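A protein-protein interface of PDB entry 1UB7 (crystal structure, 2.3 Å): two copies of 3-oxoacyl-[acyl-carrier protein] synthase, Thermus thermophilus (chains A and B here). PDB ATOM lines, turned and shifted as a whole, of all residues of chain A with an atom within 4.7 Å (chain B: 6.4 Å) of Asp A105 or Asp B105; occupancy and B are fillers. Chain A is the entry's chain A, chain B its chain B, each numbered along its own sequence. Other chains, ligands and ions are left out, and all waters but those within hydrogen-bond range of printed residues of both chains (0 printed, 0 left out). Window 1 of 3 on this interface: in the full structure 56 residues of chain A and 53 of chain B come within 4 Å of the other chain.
The backbone NH (N) of Val B77 sits at hydrogen-bond distance from the backbone carbonyl oxygen (O) of Tyr B104 (3.0 Å).
N of Ala B91 is in hydrogen-bond range of OD2 of Asp B88 (3.2 Å).
The backbone NH (N) of Thr A89 is in hydrogen-bond range of the side-chain carboxylate (OD2) of Asp A105, 2.8 Å away.
The side-chain carboxylate (OD2) of Asp A88 lies close to the backbone NH (N) of Ala A90 (3.3 Å).
The backbone NH (N) of Ala B90 sits at hydrogen-bond distance from the side-chain carboxylate (OD1) of Asp B105 (2.8 Å).
The backbone carbonyl oxygen of Val B75 lies within hydrogen-bond range of the backbone NH of Tyr B104 (3.1 Å).
Ala A90 touches none of the printed residues of chain B.
Printed residues of chain A within 4 Å of Asp B88: Leu A107 (3.2 Å).
Ala B91 touches none of the printed residues of chain A.
Of the printed residues of chain A, Tyr B104 touches Tyr A104 (3.6 Å), Leu A106 (3.5 Å) and Leu A107 (3.5 Å).
Printed residues of chain A within 4 Å of Leu B107: Asp A88, Tyr A104 and Asp A105.
Of the 19 printed residues of chain B, 6 touch a printed residue of chain A.
Printed residues of chain B that touch a printed residue of chain A: Asp B88, Tyr B104, Asp B105, Leu B106, Leu B107 and Ala B108.
Along chain A the printed residues that touch a printed residue of chain B span positions 88 to 107.
Among the printed residues, 14 pairs touch across the chains.
Among the printed residues, no Asp or Glu carboxylate lies within 4 Å of a Lys or Arg side-chain nitrogen of the other chain.
Among the printed residues, merely in contact across the chains: Asp A88 with Leu B107, Asp A88 with Ala B108, Tyr A104 with Tyr B104, Tyr A104 with Leu B106, Tyr A104 with Leu B107, Tyr A104 with Ala B108, Asp A105 with Asp B105, Asp A105 with Leu B106, Leu A106 with Tyr B104, Leu A106 with Asp B105, Leu A107 with Asp B88 and Leu A107 with Tyr B104.
Tyr B104 touches its own counterpart, Tyr A104.
Tyr A104 touches Leu B107, and with the chains exchanged Leu A107 touches Tyr B104.
Asp A105 touches its own counterpart, Asp B105.
Asp A105 touches Leu B106, and with the chains exchanged Leu A106 touches Asp B105.
The backbone carbonyl oxygen of Leu B107 lies within hydrogen-bond range of the backbone NH of Asp A105, 2.9 Å away.
The backbone carbonyl oxygen (O) of Asp B105 sits at hydrogen-bond distance from the backbone NH (N) of Leu A107 (3.0 Å).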
ATOM      1  N   VAL A  77      -2.206  20.393 -23.013  1.00  0.00           N
ATOM      2  CA  VAL A  77      -2.512  19.636 -21.803  1.00  0.00           C
ATOM      3  C   VAL A  77      -2.232  20.499 -20.573  1.00  0.00           C
ATOM      4  O   VAL A  77      -1.085  20.843 -20.283  1.00  0.00           O
ATOM      5  CB  VAL A  77      -1.672  18.339 -21.697  1.00  0.00           C
ATOM      6  CG1 VAL A  77      -1.779  17.762 -20.288  1.00  0.00           C
ATOM      7  CG2 VAL A  77      -2.174  17.296 -22.717  1.00  0.00           C
ATOM      8  N   THR A  79      -1.639  20.652 -16.996  1.00  0.00           N
ATOM      9  CA  THR A  79      -1.289  19.720 -15.934  1.00  0.00           C
ATOM     10  C   THR A  79      -0.171  20.310 -15.103  1.00  0.00           C
ATOM     11  O   THR A  79       0.456  21.292 -15.505  1.00  0.00           O
ATOM     12  CB  THR A  79      -0.798  18.367 -16.511  1.00  0.00           C
ATOM     13  OG1 THR A  79      -0.586  17.434 -15.437  1.00  0.00           O
ATOM     14  CG2 THR A  79       0.516  18.556 -17.297  1.00  0.00           C
ATOM     15  N   PRO A  82       3.160  16.383 -15.199  1.00  0.00           N
ATOM     16  CA  PRO A  82       3.432  15.703 -16.470  1.00  0.00           C
ATOM     17  C   PRO A  82       4.350  14.483 -16.291  1.00  0.00           C
ATOM     18  O   PRO A  82       5.173  14.437 -15.367  1.00  0.00           O
ATOM     19  CB  PRO A  82       4.070  16.801 -17.313  1.00  0.00           C
ATOM     20  CG  PRO A  82       4.856  17.562 -16.286  1.00  0.00           C
ATOM     21  CD  PRO A  82       3.881  17.670 -15.132  1.00  0.00           C
ATOM     22  N   ASP A  88       6.640  16.523 -23.773  1.00  0.00           N
ATOM     23  CA  ASP A  88       5.473  16.989 -23.051  1.00  0.00           C
ATOM     24  C   ASP A  88       4.330  15.992 -23.229  1.00  0.00           C
ATOM     25  O   ASP A  88       4.279  15.223 -24.181  1.00  0.00           O
ATOM     26  CB  ASP A  88       5.034  18.382 -23.529  1.00  0.00           C
ATOM     27  CG  ASP A  88       4.837  18.459 -25.045  1.00  0.00           C
ATOM     28  OD1 ASP A  88       5.847  18.527 -25.759  1.00  0.00           O
ATOM     29  OD2 ASP A  88       3.680  18.452 -25.516  1.00  0.00           O
ATOM     30  N   THR A  89       3.396  16.028 -22.305  1.00  0.00           N
ATOM     31  CA  THR A  89       2.269  15.130 -22.337  1.00  0.00           C
ATOM     32  C   THR A  89       1.360  15.421 -23.530  1.00  0.00           C
ATOM     33  O   THR A  89       0.706  14.513 -24.028  1.00  0.00           O
ATOM     34  CB  THR A  89       1.488  15.244 -21.009  1.00  0.00           C
ATOM     35  OG1 THR A  89       2.417  15.123 -19.933  1.00  0.00           O
ATOM     36  CG2 THR A  89       0.445  14.159 -20.887  1.00  0.00           C
ATOM     37  N   ALA A  90       1.310  16.671 -23.995  1.00  0.00           N
ATOM     38  CA  ALA A  90       0.452  16.985 -25.154  1.00  0.00           C
ATOM     39  C   ALA A  90       0.964  16.262 -26.383  1.00  0.00           C
ATOM     40  O   ALA A  90       0.180  15.783 -27.195  1.00  0.00           O
ATOM     41  CB  ALA A  90       0.394  18.480 -25.426  1.00  0.00           C
ATOM     42  N   TYR A 104       1.613  21.161 -26.605  1.00  0.00           N
ATOM     43  CA  TYR A 104       2.410  21.602 -25.487  1.00  0.00           C
ATOM     44  C   TYR A 104       1.679  21.481 -24.157  1.00  0.00           C
ATOM     45  O   TYR A 104       0.457  21.437 -24.118  1.00  0.00           O
ATOM     46  CB  TYR A 104       2.854  23.036 -25.723  1.00  0.00           C
ATOM     47  CG  TYR A 104       1.771  24.084 -25.578  1.00  0.00           C
ATOM     48  CD1 TYR A 104       1.398  24.562 -24.323  1.00  0.00           C
ATOM     49  CD2 TYR A 104       1.185  24.664 -26.701  1.00  0.00           C
ATOM     50  CE1 TYR A 104       0.474  25.601 -24.196  1.00  0.00           C
ATOM     51  CE2 TYR A 104       0.259  25.700 -26.584  1.00  0.00           C
ATOM     52  CZ  TYR A 104      -0.088  26.162 -25.338  1.00  0.00           C
ATOM     53  OH  TYR A 104      -0.992  27.194 -25.234  1.00  0.00           O
ATOM     54  N   ASP A 105       2.437  21.406 -23.069  1.00  0.00           N
ATOM     55  CA  ASP A 105       1.831  21.345 -21.734  1.00  0.00           C
ATOM     56  C   ASP A 105       1.800  22.757 -21.173  1.00  0.00           C
ATOM     57  O   ASP A 105       2.724  23.531 -21.383  1.00  0.00           O
ATOM     58  CB  ASP A 105       2.639  20.466 -20.766  1.00  0.00           C
ATOM     59  CG  ASP A 105       2.595  19.013 -21.136  1.00  0.00           C
ATOM     60  OD1 ASP A 105       1.728  18.663 -21.963  1.00  0.00           O
ATOM     61  OD2 ASP A 105       3.412  18.224 -20.608  1.00  0.00           O
ATOM     62  N   LEU A 106       0.734  23.080 -20.457  1.00  0.00           N
ATOM     63  CA  LEU A 106       0.586  24.384 -19.849  1.00  0.00           C
ATOM     64  C   LEU A 106       0.590  24.213 -18.310  1.00  0.00           C
ATOM     65  O   LEU A 106      -0.259  23.511 -17.750  1.00  0.00           O
ATOM     66  CB  LEU A 106      -0.725  25.016 -20.338  1.00  0.00           C
ATOM     67  CG  LEU A 106      -1.102  26.436 -19.871  1.00  0.00           C
ATOM     68  CD1 LEU A 106      -2.021  27.116 -20.903  1.00  0.00           C
ATOM     69  CD2 LEU A 106      -1.778  26.368 -18.485  1.00  0.00           C
ATOM     70  N   LEU A 107       1.558  24.829 -17.632  1.00  0.00           N
ATOM     71  CA  LEU A 107       1.615  24.741 -16.173  1.00  0.00           C
ATOM     72  C   LEU A 107       1.221  26.067 -15.534  1.00  0.00           C
ATOM     73  O   LEU A 107       1.920  27.070 -15.683  1.00  0.00           O
ATOM     74  CB  LEU A 107       3.014  24.340 -15.709  1.00  0.00           C
ATOM     75  CG  LEU A 107       3.341  22.860 -15.857  1.00  0.00           C
ATOM     76  CD1 LEU A 107       3.088  22.390 -17.285  1.00  0.00           C
ATOM     77  CD2 LEU A 107       4.763  22.648 -15.484  1.00  0.00           C
ATOM     78  N   VAL B  75       2.355  36.803 -19.092  1.00  0.00           N
ATOM     79  CA  VAL B  75       3.722  36.321 -19.091  1.00  0.00           C
ATOM     80  C   VAL B  75       3.721  34.835 -19.421  1.00  0.00           C
ATOM     81  O   VAL B  75       3.052  34.050 -18.749  1.00  0.00           O
ATOM     82  CB  VAL B  75       4.396  36.468 -17.704  1.00  0.00           C
ATOM     83  CG1 VAL B  75       5.844  35.988 -17.802  1.00  0.00           C
ATOM     84  CG2 VAL B  75       4.322  37.919 -17.216  1.00  0.00           C
ATOM     85  N   ILE B  76       4.456  34.452 -20.461  1.00  0.00           N
ATOM     86  CA  ILE B  76       4.579  33.046 -20.840  1.00  0.00           C
ATOM     87  C   ILE B  76       6.056  32.664 -20.779  1.00  0.00           C
ATOM     88  O   ILE B  76       6.901  33.305 -21.407  1.00  0.00           O
ATOM     89  CB  ILE B  76       4.103  32.759 -22.276  1.00  0.00           C
ATOM     90  CG1 ILE B  76       2.616  33.098 -22.435  1.00  0.00           C
ATOM     91  CG2 ILE B  76       4.368  31.288 -22.592  1.00  0.00           C
ATOM     92  CD1 ILE B  76       2.140  33.112 -23.888  1.00  0.00           C
ATOM     93  N   VAL B  77       6.370  31.639 -20.004  1.00  0.00           N
ATOM     94  CA  VAL B  77       7.745  31.199 -19.890  1.00  0.00           C
ATOM     95  C   VAL B  77       7.893  29.825 -20.502  1.00  0.00           C
ATOM     96  O   VAL B  77       7.394  28.827 -19.951  1.00  0.00           O
ATOM     97  CB  VAL B  77       8.212  31.131 -18.424  1.00  0.00           C
ATOM     98  CG1 VAL B  77       9.555  30.430 -18.355  1.00  0.00           C
ATOM     99  CG2 VAL B  77       8.345  32.567 -17.846  1.00  0.00           C
ATOM    100  N   ALA B  78       8.554  29.793 -21.659  1.00  0.00           N
ATOM    101  CA  ALA B  78       8.839  28.564 -22.375  1.00  0.00           C
ATOM    102  C   ALA B  78      10.102  27.963 -21.739  1.00  0.00           C
ATOM    103  O   ALA B  78      11.171  28.558 -21.778  1.00  0.00           O
ATOM    104  CB  ALA B  78       9.078  28.871 -23.837  1.00  0.00           C
ATOM    105  N   THR B  79       9.984  26.784 -21.147  1.00  0.00           N
ATOM    106  CA  THR B  79      11.128  26.169 -20.486  1.00  0.00           C
ATOM    107  C   THR B  79      10.833  24.688 -20.296  1.00  0.00           C
ATOM    108  O   THR B  79       9.688  24.252 -20.427  1.00  0.00           O
ATOM    109  CB  THR B  79      11.357  26.818 -19.081  1.00  0.00           C
ATOM    110  OG1 THR B  79      12.497  26.226 -18.439  1.00  0.00           O
ATOM    111  CG2 THR B  79      10.128  26.607 -18.202  1.00  0.00           C
ATOM    112  N   PRO B  82      11.701  24.055 -15.218  1.00  0.00           N
ATOM    113  CA  PRO B  82      11.087  25.019 -14.295  1.00  0.00           C
ATOM    114  C   PRO B  82      11.561  24.796 -12.857  1.00  0.00           C
ATOM    115  O   PRO B  82      11.885  23.664 -12.485  1.00  0.00           O
ATOM    116  CB  PRO B  82       9.599  24.757 -14.469  1.00  0.00           C
ATOM    117  CG  PRO B  82       9.563  23.256 -14.761  1.00  0.00           C
ATOM    118  CD  PRO B  82      10.730  23.041 -15.686  1.00  0.00           C
ATOM    119  N   ASP B  83      11.626  25.879 -12.076  1.00  0.00           N
ATOM    120  CA  ASP B  83      12.047  25.822 -10.675  1.00  0.00           C
ATOM    121  C   ASP B  83      11.148  24.841  -9.929  1.00  0.00           C
ATOM    122  O   ASP B  83      11.612  24.069  -9.088  1.00  0.00           O
ATOM    123  CB  ASP B  83      11.926  27.199 -10.006  1.00  0.00           C
ATOM    124  CG  ASP B  83      12.978  28.206 -10.492  1.00  0.00           C
ATOM    125  OD1 ASP B  83      13.566  27.996 -11.572  1.00  0.00           O
ATOM    126  OD2 ASP B  83      13.201  29.226  -9.794  1.00  0.00           O
ATOM    127  N   ALA B  84       9.860  24.865 -10.250  1.00  0.00           N
ATOM    128  CA  ALA B  84       8.895  23.985  -9.597  1.00  0.00           C
ATOM    129  C   ALA B  84       7.756  23.577 -10.535  1.00  0.00           C
ATOM    130  O   ALA B  84       7.550  24.186 -11.593  1.00  0.00           O
ATOM    131  CB  ALA B  84       8.310  24.691  -8.354  1.00  0.00           C
ATOM    132  N   PRO B  87       4.639  26.809  -7.728  1.00  0.00           N
ATOM    133  CA  PRO B  87       4.167  27.819  -8.679  1.00  0.00           C
ATOM    134  C   PRO B  87       4.903  27.728 -10.020  1.00  0.00           C
ATOM    135  O   PRO B  87       6.013  27.204 -10.085  1.00  0.00           O
ATOM    136  CB  PRO B  87       4.483  29.122  -7.962  1.00  0.00           C
ATOM    137  CG  PRO B  87       5.789  28.794  -7.284  1.00  0.00           C
ATOM    138  CD  PRO B  87       5.507  27.426  -6.706  1.00  0.00           C
ATOM    139  N   ASP B  88       4.279  28.216 -11.086  1.00  0.00           N
ATOM    140  CA  ASP B  88       4.940  28.206 -12.378  1.00  0.00           C
ATOM    141  C   ASP B  88       5.931  29.368 -12.414  1.00  0.00           C
ATOM    142  O   ASP B  88       5.757  30.388 -11.744  1.00  0.00           O
ATOM    143  CB  ASP B  88       3.937  28.337 -13.521  1.00  0.00           C
ATOM    144  CG  ASP B  88       2.999  29.504 -13.343  1.00  0.00           C
ATOM    145  OD1 ASP B  88       2.103  29.402 -12.480  1.00  0.00           O
ATOM    146  OD2 ASP B  88       3.160  30.521 -14.059  1.00  0.00           O
ATOM    147  N   THR B  89       6.983  29.194 -13.194  1.00  0.00           N
ATOM    148  CA  THR B  89       8.031  30.194 -13.326  1.00  0.00           C
ATOM    149  C   THR B  89       7.512  31.544 -13.815  1.00  0.00           C
ATOM    150  O   THR B  89       7.951  32.586 -13.339  1.00  0.00           O
ATOM    151  CB  THR B  89       9.100  29.664 -14.276  1.00  0.00           C
ATOM    152  OG1 THR B  89       9.382  28.306 -13.924  1.00  0.00           O
ATOM    153  CG2 THR B  89      10.379  30.496 -14.191  1.00  0.00           C
ATOM    154  N   ALA B  90       6.576  31.526 -14.763  1.00  0.00           N
ATOM    155  CA  ALA B  90       6.011  32.762 -15.299  1.00  0.00           C
ATOM    156  C   ALA B  90       5.398  33.641 -14.220  1.00  0.00           C
ATOM    157  O   ALA B  90       5.372  34.865 -14.374  1.00  0.00           O
ATOM    158  CB  ALA B  90       4.956  32.452 -16.374  1.00  0.00           C
ATOM    159  N   ALA B  91       4.898  33.025 -13.140  1.00  0.00           N
ATOM    160  CA  ALA B  91       4.264  33.776 -12.037  1.00  0.00           C
ATOM    161  C   ALA B  91       5.352  34.455 -11.225  1.00  0.00           C
ATOM    162  O   ALA B  91       5.180  35.575 -10.754  1.00  0.00           O
ATOM    163  CB  ALA B  91       3.434  32.845 -11.142  1.00  0.00           C
ATOM    164  N   ALA B 103      -0.230  34.388 -15.913  1.00  0.00           N
ATOM    165  CA  ALA B 103       1.025  33.757 -16.255  1.00  0.00           C
ATOM    166  C   ALA B 103       1.022  32.225 -16.259  1.00  0.00           C
ATOM    167  O   ALA B 103       0.269  31.583 -15.529  1.00  0.00           O
ATOM    168  CB  ALA B 103       2.088  34.265 -15.315  1.00  0.00           C
ATOM    169  N   TYR B 104       1.876  31.656 -17.102  1.00  0.00           N
ATOM    170  CA  TYR B 104       2.018  30.214 -17.204  1.00  0.00           C
ATOM    171  C   TYR B 104       3.295  29.771 -17.918  1.00  0.00           C
ATOM    172  O   TYR B 104       3.880  30.499 -18.739  1.00  0.00           O
ATOM    173  CB  TYR B 104       0.772  29.600 -17.884  1.00  0.00           C
ATOM    174  CG  TYR B 104       0.640  29.796 -19.379  1.00  0.00           C
ATOM    175  CD1 TYR B 104       1.273  28.937 -20.276  1.00  0.00           C
ATOM    176  CD2 TYR B 104      -0.165  30.806 -19.900  1.00  0.00           C
ATOM    177  CE1 TYR B 104       1.098  29.072 -21.656  1.00  0.00           C
ATOM    178  CE2 TYR B 104      -0.338  30.958 -21.285  1.00  0.00           C
ATOM    179  CZ  TYR B 104       0.293  30.083 -22.150  1.00  0.00           C
ATOM    180  OH  TYR B 104       0.095  30.199 -23.503  1.00  0.00           O
ATOM    181  N   ASP B 105       3.746  28.581 -17.568  1.00  0.00           N
ATOM    182  CA  ASP B 105       4.903  28.006 -18.213  1.00  0.00           C
ATOM    183  C   ASP B 105       4.431  27.153 -19.387  1.00  0.00           C
ATOM    184  O   ASP B 105       3.422  26.436 -19.288  1.00  0.00           O
ATOM    185  CB  ASP B 105       5.670  27.110 -17.246  1.00  0.00           C
ATOM    186  CG  ASP B 105       6.486  27.892 -16.264  1.00  0.00           C
ATOM    187  OD1 ASP B 105       6.305  29.129 -16.184  1.00  0.00           O
ATOM    188  OD2 ASP B 105       7.306  27.261 -15.567  1.00  0.00           O
ATOM    189  N   LEU B 106       5.177  27.219 -20.488  1.00  0.00           N
ATOM    190  CA  LEU B 106       4.856  26.433 -21.676  1.00  0.00           C
ATOM    191  C   LEU B 106       5.951  25.386 -21.889  1.00  0.00           C
ATOM    192  O   LEU B 106       7.133  25.713 -21.975  1.00  0.00           O
ATOM    193  CB  LEU B 106       4.718  27.363 -22.895  1.00  0.00           C
ATOM    194  CG  LEU B 106       4.225  26.727 -24.205  1.00  0.00           C
ATOM    195  CD1 LEU B 106       3.657  27.800 -25.098  1.00  0.00           C
ATOM    196  CD2 LEU B 106       5.347  25.996 -24.895  1.00  0.00           C
ATOM    197  N   LEU B 107       5.559  24.121 -21.939  1.00  0.00           N
ATOM    198  CA  LEU B 107       6.508  23.027 -22.137  1.00  0.00           C
ATOM    199  C   LEU B 107       6.301  22.382 -23.501  1.00  0.00           C
ATOM    200  O   LEU B 107       5.277  21.736 -23.745  1.00  0.00           O
ATOM    201  CB  LEU B 107       6.338  21.952 -21.044  1.00  0.00           C
ATOM    202  CG  LEU B 107       7.067  22.169 -19.722  1.00  0.00           C
ATOM    203  CD1 LEU B 107       6.749  23.563 -19.142  1.00  0.00           C
ATOM    204  CD2 LEU B 107       6.660  21.058 -18.763  1.00  0.00           C
ATOM    205  N   ALA B 108       7.281  22.551 -24.379  1.00  0.00           N
ATOM    206  CA  ALA B 108       7.215  21.999 -25.728  1.00  0.00           C
ATOM    207  C   ALA B 108       8.623  21.746 -26.275  1.00  0.00           C
ATOM    208  O   ALA B 108       8.872  21.922 -27.463  1.00  0.00           O
ATOM    209  CB  ALA B 108       6.445  22.971 -26.659  1.00  0.00           C
